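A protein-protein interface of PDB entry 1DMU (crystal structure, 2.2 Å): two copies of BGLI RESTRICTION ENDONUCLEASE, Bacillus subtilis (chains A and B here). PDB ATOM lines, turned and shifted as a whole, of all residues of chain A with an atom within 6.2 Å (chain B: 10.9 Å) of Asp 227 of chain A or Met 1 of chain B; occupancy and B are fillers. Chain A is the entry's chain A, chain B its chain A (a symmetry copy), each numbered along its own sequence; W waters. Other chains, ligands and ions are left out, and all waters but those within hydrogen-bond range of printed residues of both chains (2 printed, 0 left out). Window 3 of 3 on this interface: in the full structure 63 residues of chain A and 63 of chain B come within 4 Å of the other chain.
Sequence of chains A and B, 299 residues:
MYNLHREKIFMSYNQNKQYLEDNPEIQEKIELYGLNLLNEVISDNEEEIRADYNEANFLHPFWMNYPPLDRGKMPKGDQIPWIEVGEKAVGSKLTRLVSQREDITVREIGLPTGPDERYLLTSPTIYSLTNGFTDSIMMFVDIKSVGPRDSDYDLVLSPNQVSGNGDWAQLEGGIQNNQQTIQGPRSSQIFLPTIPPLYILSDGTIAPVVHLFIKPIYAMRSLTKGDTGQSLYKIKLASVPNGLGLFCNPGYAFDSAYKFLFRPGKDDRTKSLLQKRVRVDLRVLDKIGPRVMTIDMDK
The side-chain carboxylate (OE1) of Glu 55 of chain A lies within hydrogen-bond range of the side-chain hydroxyl (OG) of Ser 202 of chain B, 2.6 Å away. The side-chain hydroxyl (OG1) of Thr 228 of chain A lies within hydrogen-bond range of the backbone NH (N) of Tyr 2 of chain B, 3.0 Å away. The backbone NH (N) of Met 1 of chain B is in hydrogen-bond range of the side-chain hydroxyl (OG1) of Thr 228 of chain A (2.8 Å). ND2 of Asn 57 of chain A lies within hydrogen-bond range of SD of Met 1 of chain B (3.6 Å).
The guanidinium group (NH1) of Arg 221 of chain A is in hydrogen-bond range of the side-chain hydroxyl (OG) of Ser 231 of chain A. O of Tyr 2 of chain B lies within hydrogen-bond range of NH1 of Arg 6 of chain B (3.0 Å). The side-chain amide oxygen (OD1) of Asn 57 of chain A lies within hydrogen-bond range of the backbone NH (N) of Gln 230 of chain A (2.8 Å). The backbone NH (N) of Arg 221 of chain A is in hydrogen-bond range of the backbone carbonyl oxygen (O) of Gly 229 of chain A, 2.9 Å away. N of Ser 222 of chain A lies close to O of Asp 227 of chain A. The side-chain carboxylate of Asp 227 of chain A is in salt-bridge range of the guanidinium group of Arg 221 of chain A, at 3.7 Å.
Among the printed residues, pairs that only touch across the chains: Asn 54 of chain A with Met 1 of chain B (3.8 Å), Glu 55 of chain A with Leu 201 of chain B (3.5 Å), Asn 57 of chain A with Tyr 2 of chain B (3.3 Å), Phe 58 of chain A with Met 1 of chain B (3.3 Å), Phe 58 of chain A with Leu 4 of chain B (3.97 Å), Phe 58 of chain A with His 5 of chain B (3.9 Å), Phe 58 of chain A with Ile 9 of chain B (3.6 Å), Phe 58 of chain A with Ser 202 of chain B (3.8 Å), Arg 221 of chain A with Met 1 of chain B (3.8 Å), Asp 227 of chain A with Met 1 of chain B (3.9 Å), Gly 229 of chain A with Tyr 2 of chain B (3.9 Å) and Ser 231 of chain A with Met 1 of chain B (3.9 Å).
Met 1 of chain B touches seven residues of chain A. Asn 57 of chain A touches just these residues of chain B: Met 1 (3.6 Å) and Tyr 2 (3.3 Å). Phe 58 of chain A touches five residues of chain B. No residue of chain B comes within 4 Å of Ser 222 of chain A. No residue of chain B comes within 4 Å of Lys 225 of chain A. No residue of chain B comes within 4 Å of Gly 226 of chain A. Thr 228 of chain A touches just these residues of chain B: Met 1 (2.8 Å) and Tyr 2 (3.0 Å). Printed residues of chain A within 4 Å of Leu 201 of chain B: Glu 55. Of the printed residues of chain B, Ser 231 of chain A touches Met 1 (3.9 Å). Printed residues of chain A within 4 Å of Leu 4 of chain B: Phe 58 (3.97 Å). Gln 230 of chain A touches none of the printed residues of chain B. Leu 171 of chain B touches none of the printed residues of chain A. The nearest residue of chain B that does not touch Asp 227 of chain A is Tyr 2 of chain B (6.4 Å). The nearest printed residue of chain B that does not touch Glu 55 of chain A is Gly 110 of chain B (4.2 Å).
Hydrophobic or aromatic side chains of chain A that line the printed part of chain B: Phe 58. Of the 15 printed residues of chain B, 7 touch a printed residue of chain A. Hydrophobic or aromatic side chains of chain B within 4 Å of the printed part of chain A: Met 1, Tyr 2, Leu 4, His 5, Ile 9 and Leu 201. Among the printed residues, 16 pairs touch across the chains. Among the printed residues, no Asp or Glu carboxylate lies within 4 Å of a Lys or Arg side-chain nitrogen of the other chain.
No position is printed for both chains.
Water W2 lies within hydrogen-bond range of O of Tyr 2 of chain B, O of Phe 58 of chain A and N of Arg 6 of chain B. Water W1 bridges OH of Tyr 2 of chain B (2.8 Å) and N of Gly 229 of chain A (2.8 Å).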
ATOM      1  N   ASN A  54      -4.430  -5.499  -9.481  1.00  0.00           N
ATOM      2  CA  ASN A  54      -4.074  -5.313  -8.078  1.00  0.00           C
ATOM      3  C   ASN A  54      -2.905  -6.146  -7.586  1.00  0.00           C
ATOM      4  O   ASN A  54      -2.285  -5.795  -6.584  1.00  0.00           O
ATOM      5  CB  ASN A  54      -5.296  -5.580  -7.206  1.00  0.00           C
ATOM      6  CG  ASN A  54      -6.343  -4.512  -7.360  1.00  0.00           C
ATOM      7  OD1 ASN A  54      -6.075  -3.444  -7.905  1.00  0.00           O
ATOM      8  ND2 ASN A  54      -7.542  -4.782  -6.877  1.00  0.00           N
ATOM      9  N   GLU A  55      -2.606  -7.239  -8.287  1.00  0.00           N
ATOM     10  CA  GLU A  55      -1.491  -8.123  -7.918  1.00  0.00           C
ATOM     11  C   GLU A  55      -0.149  -7.372  -7.882  1.00  0.00           C
ATOM     12  O   GLU A  55       0.760  -7.749  -7.140  1.00  0.00           O
ATOM     13  CB  GLU A  55      -1.409  -9.323  -8.887  1.00  0.00           C
ATOM     14  CG  GLU A  55      -0.388 -10.429  -8.522  1.00  0.00           C
ATOM     15  CD  GLU A  55      -0.645 -11.130  -7.187  1.00  0.00           C
ATOM     16  OE1 GLU A  55      -1.786 -11.102  -6.677  1.00  0.00           O
ATOM     17  OE2 GLU A  55       0.315 -11.720  -6.638  1.00  0.00           O
ATOM     18  N   ASN A  57       0.560  -4.665  -6.510  1.00  0.00           N
ATOM     19  CA  ASN A  57       0.748  -4.149  -5.146  1.00  0.00           C
ATOM     20  C   ASN A  57       1.225  -5.225  -4.173  1.00  0.00           C
ATOM     21  O   ASN A  57       2.000  -4.940  -3.254  1.00  0.00           O
ATOM     22  CB  ASN A  57      -0.562  -3.591  -4.606  1.00  0.00           C
ATOM     23  CG  ASN A  57      -1.103  -2.459  -5.444  1.00  0.00           C
ATOM     24  OD1 ASN A  57      -0.544  -1.354  -5.456  1.00  0.00           O
ATOM     25  ND2 ASN A  57      -2.202  -2.719  -6.143  1.00  0.00           N
ATOM     26  N   PHE A  58       0.732  -6.449  -4.363  1.00  0.00           N
ATOM     27  CA  PHE A  58       1.106  -7.568  -3.511  1.00  0.00           C
ATOM     28  C   PHE A  58       2.556  -7.966  -3.819  1.00  0.00           C
ATOM     29  O   PHE A  58       3.288  -8.455  -2.942  1.00  0.00           O
ATOM     30  CB  PHE A  58       0.136  -8.737  -3.748  1.00  0.00           C
ATOM     31  CG  PHE A  58      -1.310  -8.408  -3.413  1.00  0.00           C
ATOM     32  CD1 PHE A  58      -2.357  -8.972  -4.141  1.00  0.00           C
ATOM     33  CD2 PHE A  58      -1.625  -7.550  -2.367  1.00  0.00           C
ATOM     34  CE1 PHE A  58      -3.676  -8.692  -3.833  1.00  0.00           C
ATOM     35  CE2 PHE A  58      -2.957  -7.262  -2.053  1.00  0.00           C
ATOM     36  CZ  PHE A  58      -3.977  -7.837  -2.787  1.00  0.00           C
ATOM     37  N   ARG A 221      -4.570   4.156  -1.978  1.00  0.00           N
ATOM     38  CA  ARG A 221      -4.924   3.703  -0.628  1.00  0.00           C
ATOM     39  C   ARG A 221      -4.210   4.488   0.470  1.00  0.00           C
ATOM     40  O   ARG A 221      -4.765   4.749   1.524  1.00  0.00           O
ATOM     41  CB  ARG A 221      -4.606   2.216  -0.471  1.00  0.00           C
ATOM     42  CG  ARG A 221      -5.244   1.343  -1.529  1.00  0.00           C
ATOM     43  CD  ARG A 221      -6.593   0.878  -1.075  1.00  0.00           C
ATOM     44  NE  ARG A 221      -6.654  -0.570  -0.959  1.00  0.00           N
ATOM     45  CZ  ARG A 221      -7.554  -1.314  -1.592  1.00  0.00           C
ATOM     46  NH1 ARG A 221      -8.450  -0.730  -2.372  1.00  0.00           N
ATOM     47  NH2 ARG A 221      -7.553  -2.638  -1.455  1.00  0.00           N
ATOM     48  N   SER A 222      -2.970   4.858   0.200  1.00  0.00           N
ATOM     49  CA  SER A 222      -2.154   5.614   1.138  1.00  0.00           C
ATOM     50  C   SER A 222      -2.820   6.924   1.521  1.00  0.00           C
ATOM     51  O   SER A 222      -2.455   7.525   2.525  1.00  0.00           O
ATOM     52  CB  SER A 222      -0.793   5.922   0.515  1.00  0.00           C
ATOM     53  OG  SER A 222      -0.885   7.105  -0.261  1.00  0.00           O
ATOM     54  N   LEU A 223      -3.773   7.391   0.717  1.00  0.00           N
ATOM     55  CA  LEU A 223      -4.450   8.639   1.048  1.00  0.00           C
ATOM     56  C   LEU A 223      -5.234   8.428   2.341  1.00  0.00           C
ATOM     57  O   LEU A 223      -5.713   9.382   2.949  1.00  0.00           O
ATOM     58  CB  LEU A 223      -5.386   9.078  -0.083  1.00  0.00           C
ATOM     59  CG  LEU A 223      -4.742   9.811  -1.272  1.00  0.00           C
ATOM     60  CD1 LEU A 223      -5.817  10.485  -2.101  1.00  0.00           C
ATOM     61  CD2 LEU A 223      -3.725  10.830  -0.777  1.00  0.00           C
ATOM     62  N   THR A 224      -5.358   7.164   2.750  1.00  0.00           N
ATOM     63  CA  THR A 224      -6.051   6.793   3.987  1.00  0.00           C
ATOM     64  C   THR A 224      -4.981   6.269   4.944  1.00  0.00           C
ATOM     65  O   THR A 224      -4.335   5.244   4.683  1.00  0.00           O
ATOM     66  CB  THR A 224      -7.101   5.716   3.729  1.00  0.00           C
ATOM     67  N   LYS A 225      -4.791   7.006   6.037  1.00  0.00           N
ATOM     68  CA  LYS A 225      -3.806   6.699   7.081  1.00  0.00           C
ATOM     69  C   LYS A 225      -3.347   5.240   7.185  1.00  0.00           C
ATOM     70  O   LYS A 225      -4.134   4.343   7.498  1.00  0.00           O
ATOM     71  CB  LYS A 225      -4.344   7.166   8.451  1.00  0.00           C
ATOM     72  N   GLY A 226      -2.063   5.024   6.906  1.00  0.00           N
ATOM     73  CA  GLY A 226      -1.461   3.701   7.016  1.00  0.00           C
ATOM     74  C   GLY A 226      -1.854   2.596   6.046  1.00  0.00           C
ATOM     75  O   GLY A 226      -1.355   1.468   6.170  1.00  0.00           O
ATOM     76  N   ASP A 227      -2.748   2.874   5.099  1.00  0.00           N
ATOM     77  CA  ASP A 227      -3.116   1.844   4.123  1.00  0.00           C
ATOM     78  C   ASP A 227      -2.153   1.980   2.931  1.00  0.00           C
ATOM     79  O   ASP A 227      -1.582   3.046   2.714  1.00  0.00           O
ATOM     80  CB  ASP A 227      -4.570   2.012   3.694  1.00  0.00           C
ATOM     81  CG  ASP A 227      -5.103   0.802   2.950  1.00  0.00           C
ATOM     82  OD1 ASP A 227      -4.396  -0.234   2.884  1.00  0.00           O
ATOM     83  OD2 ASP A 227      -6.236   0.896   2.424  1.00  0.00           O
ATOM     84  N   THR A 228      -1.967   0.921   2.151  1.00  0.00           N
ATOM     85  CA  THR A 228      -1.016   0.993   1.044  1.00  0.00           C
ATOM     86  C   THR A 228      -1.529   0.394  -0.249  1.00  0.00           C
ATOM     87  O   THR A 228      -2.436  -0.427  -0.246  1.00  0.00           O
ATOM     88  CB  THR A 228       0.302   0.241   1.388  1.00  0.00           C
ATOM     89  OG1 THR A 228      -0.011  -1.117   1.716  1.00  0.00           O
ATOM     90  CG2 THR A 228       1.024   0.890   2.571  1.00  0.00           C
ATOM     91  N   GLY A 229      -0.915   0.813  -1.356  1.00  0.00           N
ATOM     92  CA  GLY A 229      -1.273   0.304  -2.670  1.00  0.00           C
ATOM     93  C   GLY A 229      -2.103   1.213  -3.559  1.00  0.00           C
ATOM     94  O   GLY A 229      -2.763   2.145  -3.108  1.00  0.00           O
ATOM     95  N   GLN A 230      -2.065   0.916  -4.852  1.00  0.00           N
ATOM     96  CA  GLN A 230      -2.813   1.656  -5.863  1.00  0.00           C
ATOM     97  C   GLN A 230      -3.684   0.617  -6.575  1.00  0.00           C
ATOM     98  O   GLN A 230      -3.246  -0.059  -7.510  1.00  0.00           O
ATOM     99  CB  GLN A 230      -1.821   2.343  -6.814  1.00  0.00           C
ATOM    100  CG  GLN A 230      -1.273   3.658  -6.236  1.00  0.00           C
ATOM    101  CD  GLN A 230       0.049   4.095  -6.839  1.00  0.00           C
ATOM    102  OE1 GLN A 230       0.791   4.853  -6.212  1.00  0.00           O
ATOM    103  NE2 GLN A 230       0.349   3.647  -8.052  1.00  0.00           N
ATOM    104  N   SER A 231      -4.923   0.502  -6.112  1.00  0.00           N
ATOM    105  CA  SER A 231      -5.862  -0.492  -6.611  1.00  0.00           C
ATOM    106  C   SER A 231      -6.808  -0.056  -7.735  1.00  0.00           C
ATOM    107  O   SER A 231      -7.134   1.118  -7.862  1.00  0.00           O
ATOM    108  CB  SER A 231      -6.678  -0.972  -5.424  1.00  0.00           C
ATOM    109  OG  SER A 231      -7.129   0.156  -4.686  1.00  0.00           O
ATOM    110  N   MET B   1      -2.124  -2.863   1.185  1.00  0.00           N
ATOM    111  CA  MET B   1      -2.016  -4.074   0.316  1.00  0.00           C
ATOM    112  C   MET B   1      -0.618  -4.669   0.354  1.00  0.00           C
ATOM    113  O   MET B   1      -0.451  -5.880   0.208  1.00  0.00           O
ATOM    114  CB  MET B   1      -2.358  -3.721  -1.134  1.00  0.00           C
ATOM    115  CG  MET B   1      -3.756  -3.156  -1.336  1.00  0.00           C
ATOM    116  SD  MET B   1      -4.048  -2.678  -3.058  1.00  0.00           S
ATOM    117  CE  MET B   1      -4.458  -4.210  -3.755  1.00  0.00           C
ATOM    118  N   TYR B   2       0.372  -3.805   0.553  1.00  0.00           N
ATOM    119  CA  TYR B   2       1.779  -4.200   0.579  1.00  0.00           C
ATOM    120  C   TYR B   2       2.135  -5.287   1.594  1.00  0.00           C
ATOM    121  O   TYR B   2       3.027  -6.119   1.347  1.00  0.00           O
ATOM    122  CB  TYR B   2       2.668  -2.978   0.858  1.00  0.00           C
ATOM    123  CG  TYR B   2       2.730  -1.937  -0.247  1.00  0.00           C
ATOM    124  CD1 TYR B   2       2.209  -2.192  -1.514  1.00  0.00           C
ATOM    125  CD2 TYR B   2       3.314  -0.689  -0.019  1.00  0.00           C
ATOM    126  CE1 TYR B   2       2.270  -1.223  -2.524  1.00  0.00           C
ATOM    127  CE2 TYR B   2       3.377   0.271  -1.015  1.00  0.00           C
ATOM    128  CZ  TYR B   2       2.853   0.001  -2.264  1.00  0.00           C
ATOM    129  OH  TYR B   2       2.896   0.961  -3.254  1.00  0.00           O
ATOM    130  N   ASN B   3       1.428  -5.295   2.719  1.00  0.00           N
ATOM    131  CA  ASN B   3       1.719  -6.242   3.781  1.00  0.00           C
ATOM    132  C   ASN B   3       0.788  -7.447   3.925  1.00  0.00           C
ATOM    133  O   ASN B   3       1.140  -8.411   4.602  1.00  0.00           O
ATOM    134  CB  ASN B   3       1.789  -5.481   5.118  1.00  0.00           C
ATOM    135  CG  ASN B   3       2.939  -4.472   5.156  1.00  0.00           C
ATOM    136  OD1 ASN B   3       3.994  -4.676   4.538  1.00  0.00           O
ATOM    137  ND2 ASN B   3       2.737  -3.376   5.876  1.00  0.00           N
ATOM    138  N   LEU B   4      -0.371  -7.392   3.276  1.00  0.00           N
ATOM    139  CA  LEU B   4      -1.396  -8.444   3.355  1.00  0.00           C
ATOM    140  C   LEU B   4      -0.951  -9.894   3.129  1.00  0.00           C
ATOM    141  O   LEU B   4      -1.421 -10.802   3.803  1.00  0.00           O
ATOM    142  CB  LEU B   4      -2.536  -8.110   2.392  1.00  0.00           C
ATOM    143  CG  LEU B   4      -3.733  -9.056   2.372  1.00  0.00           C
ATOM    144  CD1 LEU B   4      -4.438  -9.020   3.721  1.00  0.00           C
ATOM    145  CD2 LEU B   4      -4.680  -8.643   1.247  1.00  0.00           C
ATOM    146  N   HIS B   5      -0.063 -10.128   2.177  1.00  0.00           N
ATOM    147  CA  HIS B   5       0.390 -11.484   1.935  1.00  0.00           C
ATOM    148  C   HIS B   5       1.892 -11.526   2.018  1.00  0.00           C
ATOM    149  O   HIS B   5       2.495 -12.541   1.694  1.00  0.00           O
ATOM    150  CB  HIS B   5      -0.023 -11.961   0.544  1.00  0.00           C
ATOM    151  CG  HIS B   5      -1.487 -11.840   0.273  1.00  0.00           C
ATOM    152  ND1 HIS B   5      -2.429 -12.664   0.866  1.00  0.00           N
ATOM    153  CD2 HIS B   5      -2.185 -10.976  -0.498  1.00  0.00           C
ATOM    154  CE1 HIS B   5      -3.631 -12.306   0.471  1.00  0.00           C
ATOM    155  NE2 HIS B   5      -3.516 -11.279  -0.360  1.00  0.00           N
ATOM    156  N   ARG B   6       2.488 -10.423   2.465  1.00  0.00           N
ATOM    157  CA  ARG B   6       3.930 -10.305   2.543  1.00  0.00           C
ATOM    158  C   ARG B   6       4.668 -11.435   3.243  1.00  0.00           C
ATOM    159  O   ARG B   6       5.653 -11.945   2.703  1.00  0.00           O
ATOM    160  CB  ARG B   6       4.326  -8.957   3.166  1.00  0.00           C
ATOM    161  CG  ARG B   6       5.622  -8.397   2.573  1.00  0.00           C
ATOM    162  CD  ARG B   6       6.232  -7.301   3.433  1.00  0.00           C
ATOM    163  NE  ARG B   6       7.308  -6.603   2.731  1.00  0.00           N
ATOM    164  CZ  ARG B   6       7.129  -5.686   1.782  1.00  0.00           C
ATOM    165  NH1 ARG B   6       5.907  -5.335   1.388  1.00  0.00           N
ATOM    166  NH2 ARG B   6       8.180  -5.136   1.200  1.00  0.00           N
ATOM    167  N   GLU B   7       4.214 -11.836   4.430  1.00  0.00           N
ATOM    168  CA  GLU B   7       4.889 -12.906   5.167  1.00  0.00           C
ATOM    169  C   GLU B   7       4.899 -14.211   4.380  1.00  0.00           C
ATOM    170  O   GLU B   7       5.922 -14.888   4.288  1.00  0.00           O
ATOM    171  CB  GLU B   7       4.228 -13.113   6.536  1.00  0.00           C
ATOM    172  N   LYS B   8       3.763 -14.556   3.790  1.00  0.00           N
ATOM    173  CA  LYS B   8       3.674 -15.791   3.030  1.00  0.00           C
ATOM    174  C   LYS B   8       4.570 -15.749   1.791  1.00  0.00           C
ATOM    175  O   LYS B   8       5.170 -16.759   1.426  1.00  0.00           O
ATOM    176  CB  LYS B   8       2.226 -16.061   2.620  1.00  0.00           C
ATOM    177  CG  LYS B   8       2.046 -17.336   1.787  1.00  0.00           C
ATOM    178  CD  LYS B   8       0.632 -17.455   1.207  1.00  0.00           C
ATOM    179  CE  LYS B   8       0.463 -18.801   0.492  1.00  0.00           C
ATOM    180  NZ  LYS B   8      -0.932 -19.051   0.014  1.00  0.00           N
ATOM    181  N   ILE B   9       4.656 -14.589   1.139  1.00  0.00           N
ATOM    182  CA  ILE B   9       5.486 -14.451  -0.059  1.00  0.00           C
ATOM    183  C   ILE B   9       6.959 -14.525   0.342  1.00  0.00           C
ATOM    184  O   ILE B   9       7.768 -15.189  -0.309  1.00  0.00           O
ATOM    185  CB  ILE B   9       5.170 -13.104  -0.793  1.00  0.00           C
ATOM    186  CG1 ILE B   9       3.793 -13.210  -1.458  1.00  0.00           C
ATOM    187  CG2 ILE B   9       6.214 -12.798  -1.864  1.00  0.00           C
ATOM    188  CD1 ILE B   9       3.170 -11.860  -1.837  1.00  0.00           C
ATOM    189  N   GLY B 110       0.052  -8.005 -13.224  1.00  0.00           N
ATOM    190  CA  GLY B 110       0.493  -6.624 -13.207  1.00  0.00           C
ATOM    191  C   GLY B 110       1.839  -6.407 -12.531  1.00  0.00           C
ATOM    192  O   GLY B 110       2.084  -6.929 -11.446  1.00  0.00           O
ATOM    193  N   TRP B 168      16.659 -11.132  -0.111  1.00  0.00           N
ATOM    194  CA  TRP B 168      15.573 -10.461   0.590  1.00  0.00           C
ATOM    195  C   TRP B 168      15.836 -10.791   2.063  1.00  0.00           C
ATOM    196  O   TRP B 168      15.345 -11.785   2.593  1.00  0.00           O
ATOM    197  CB  TRP B 168      14.214 -11.004   0.100  1.00  0.00           C
ATOM    198  CG  TRP B 168      12.977 -10.343   0.713  1.00  0.00           C
ATOM    199  CD1 TRP B 168      12.956  -9.407   1.703  1.00  0.00           C
ATOM    200  CD2 TRP B 168      11.591 -10.629   0.401  1.00  0.00           C
ATOM    201  NE1 TRP B 168      11.654  -9.094   2.036  1.00  0.00           N
ATOM    202  CE2 TRP B 168      10.799  -9.826   1.255  1.00  0.00           C
ATOM    203  CE3 TRP B 168      10.949 -11.488  -0.515  1.00  0.00           C
ATOM    204  CZ2 TRP B 168       9.387  -9.853   1.229  1.00  0.00           C
ATOM    205  CZ3 TRP B 168       9.544 -11.519  -0.541  1.00  0.00           C
ATOM    206  CH2 TRP B 168       8.782 -10.703   0.329  1.00  0.00           C
ATOM    207  N   LEU B 171      11.711  -9.120   6.196  1.00  0.00           N
ATOM    208  CA  LEU B 171      10.325  -9.061   5.738  1.00  0.00           C
ATOM    209  C   LEU B 171       9.823  -7.675   5.326  1.00  0.00           C
ATOM    210  O   LEU B 171       9.296  -7.514   4.229  1.00  0.00           O
ATOM    211  CB  LEU B 171       9.409  -9.627   6.823  1.00  0.00           C
ATOM    212  CG  LEU B 171       7.909  -9.488   6.575  1.00  0.00           C
ATOM    213  CD1 LEU B 171       7.387 -10.601   5.674  1.00  0.00           C
ATOM    214  CD2 LEU B 171       7.232  -9.498   7.900  1.00  0.00           C
ATOM    215  N   ILE B 200       6.872 -14.846  -6.361  1.00  0.00           N
ATOM    216  CA  ILE B 200       5.921 -15.708  -5.649  1.00  0.00           C
ATOM    217  C   ILE B 200       4.657 -14.842  -5.655  1.00  0.00           C
ATOM    218  O   ILE B 200       4.693 -13.697  -5.198  1.00  0.00           O
ATOM    219  CB  ILE B 200       6.322 -16.026  -4.181  1.00  0.00           C
ATOM    220  CG1 ILE B 200       7.675 -16.730  -4.140  1.00  0.00           C
ATOM    221  CG2 ILE B 200       5.289 -16.959  -3.547  1.00  0.00           C
ATOM    222  CD1 ILE B 200       7.669 -18.099  -4.792  1.00  0.00           C
ATOM    223  N   LEU B 201       3.565 -15.351  -6.224  1.00  0.00           N
ATOM    224  CA  LEU B 201       2.334 -14.570  -6.254  1.00  0.00           C
ATOM    225  C   LEU B 201       1.580 -14.667  -4.933  1.00  0.00           C
ATOM    226  O   LEU B 201       1.833 -15.563  -4.131  1.00  0.00           O
ATOM    227  CB  LEU B 201       1.454 -15.017  -7.436  1.00  0.00           C
ATOM    228  CG  LEU B 201       2.258 -15.072  -8.759  1.00  0.00           C
ATOM    229  CD1 LEU B 201       1.371 -15.591  -9.862  1.00  0.00           C
ATOM    230  CD2 LEU B 201       2.862 -13.696  -9.126  1.00  0.00           C
ATOM    231  N   SER B 202       0.662 -13.736  -4.699  1.00  0.00           N
ATOM    232  CA  SER B 202      -0.110 -13.719  -3.470  1.00  0.00           C
ATOM    233  C   SER B 202      -0.845 -15.035  -3.163  1.00  0.00           C
ATOM    234  O   SER B 202      -1.325 -15.240  -2.047  1.00  0.00           O
ATOM    235  CB  SER B 202      -1.110 -12.560  -3.507  1.00  0.00           C
ATOM    236  OG  SER B 202      -1.991 -12.699  -4.591  1.00  0.00           O
HETATM  237  O   HOH W   1       1.028   2.667  -2.174  1.00  0.00           O
HETATM  238  O   HOH W   2       3.474  -8.323  -0.065  1.00  0.00           O
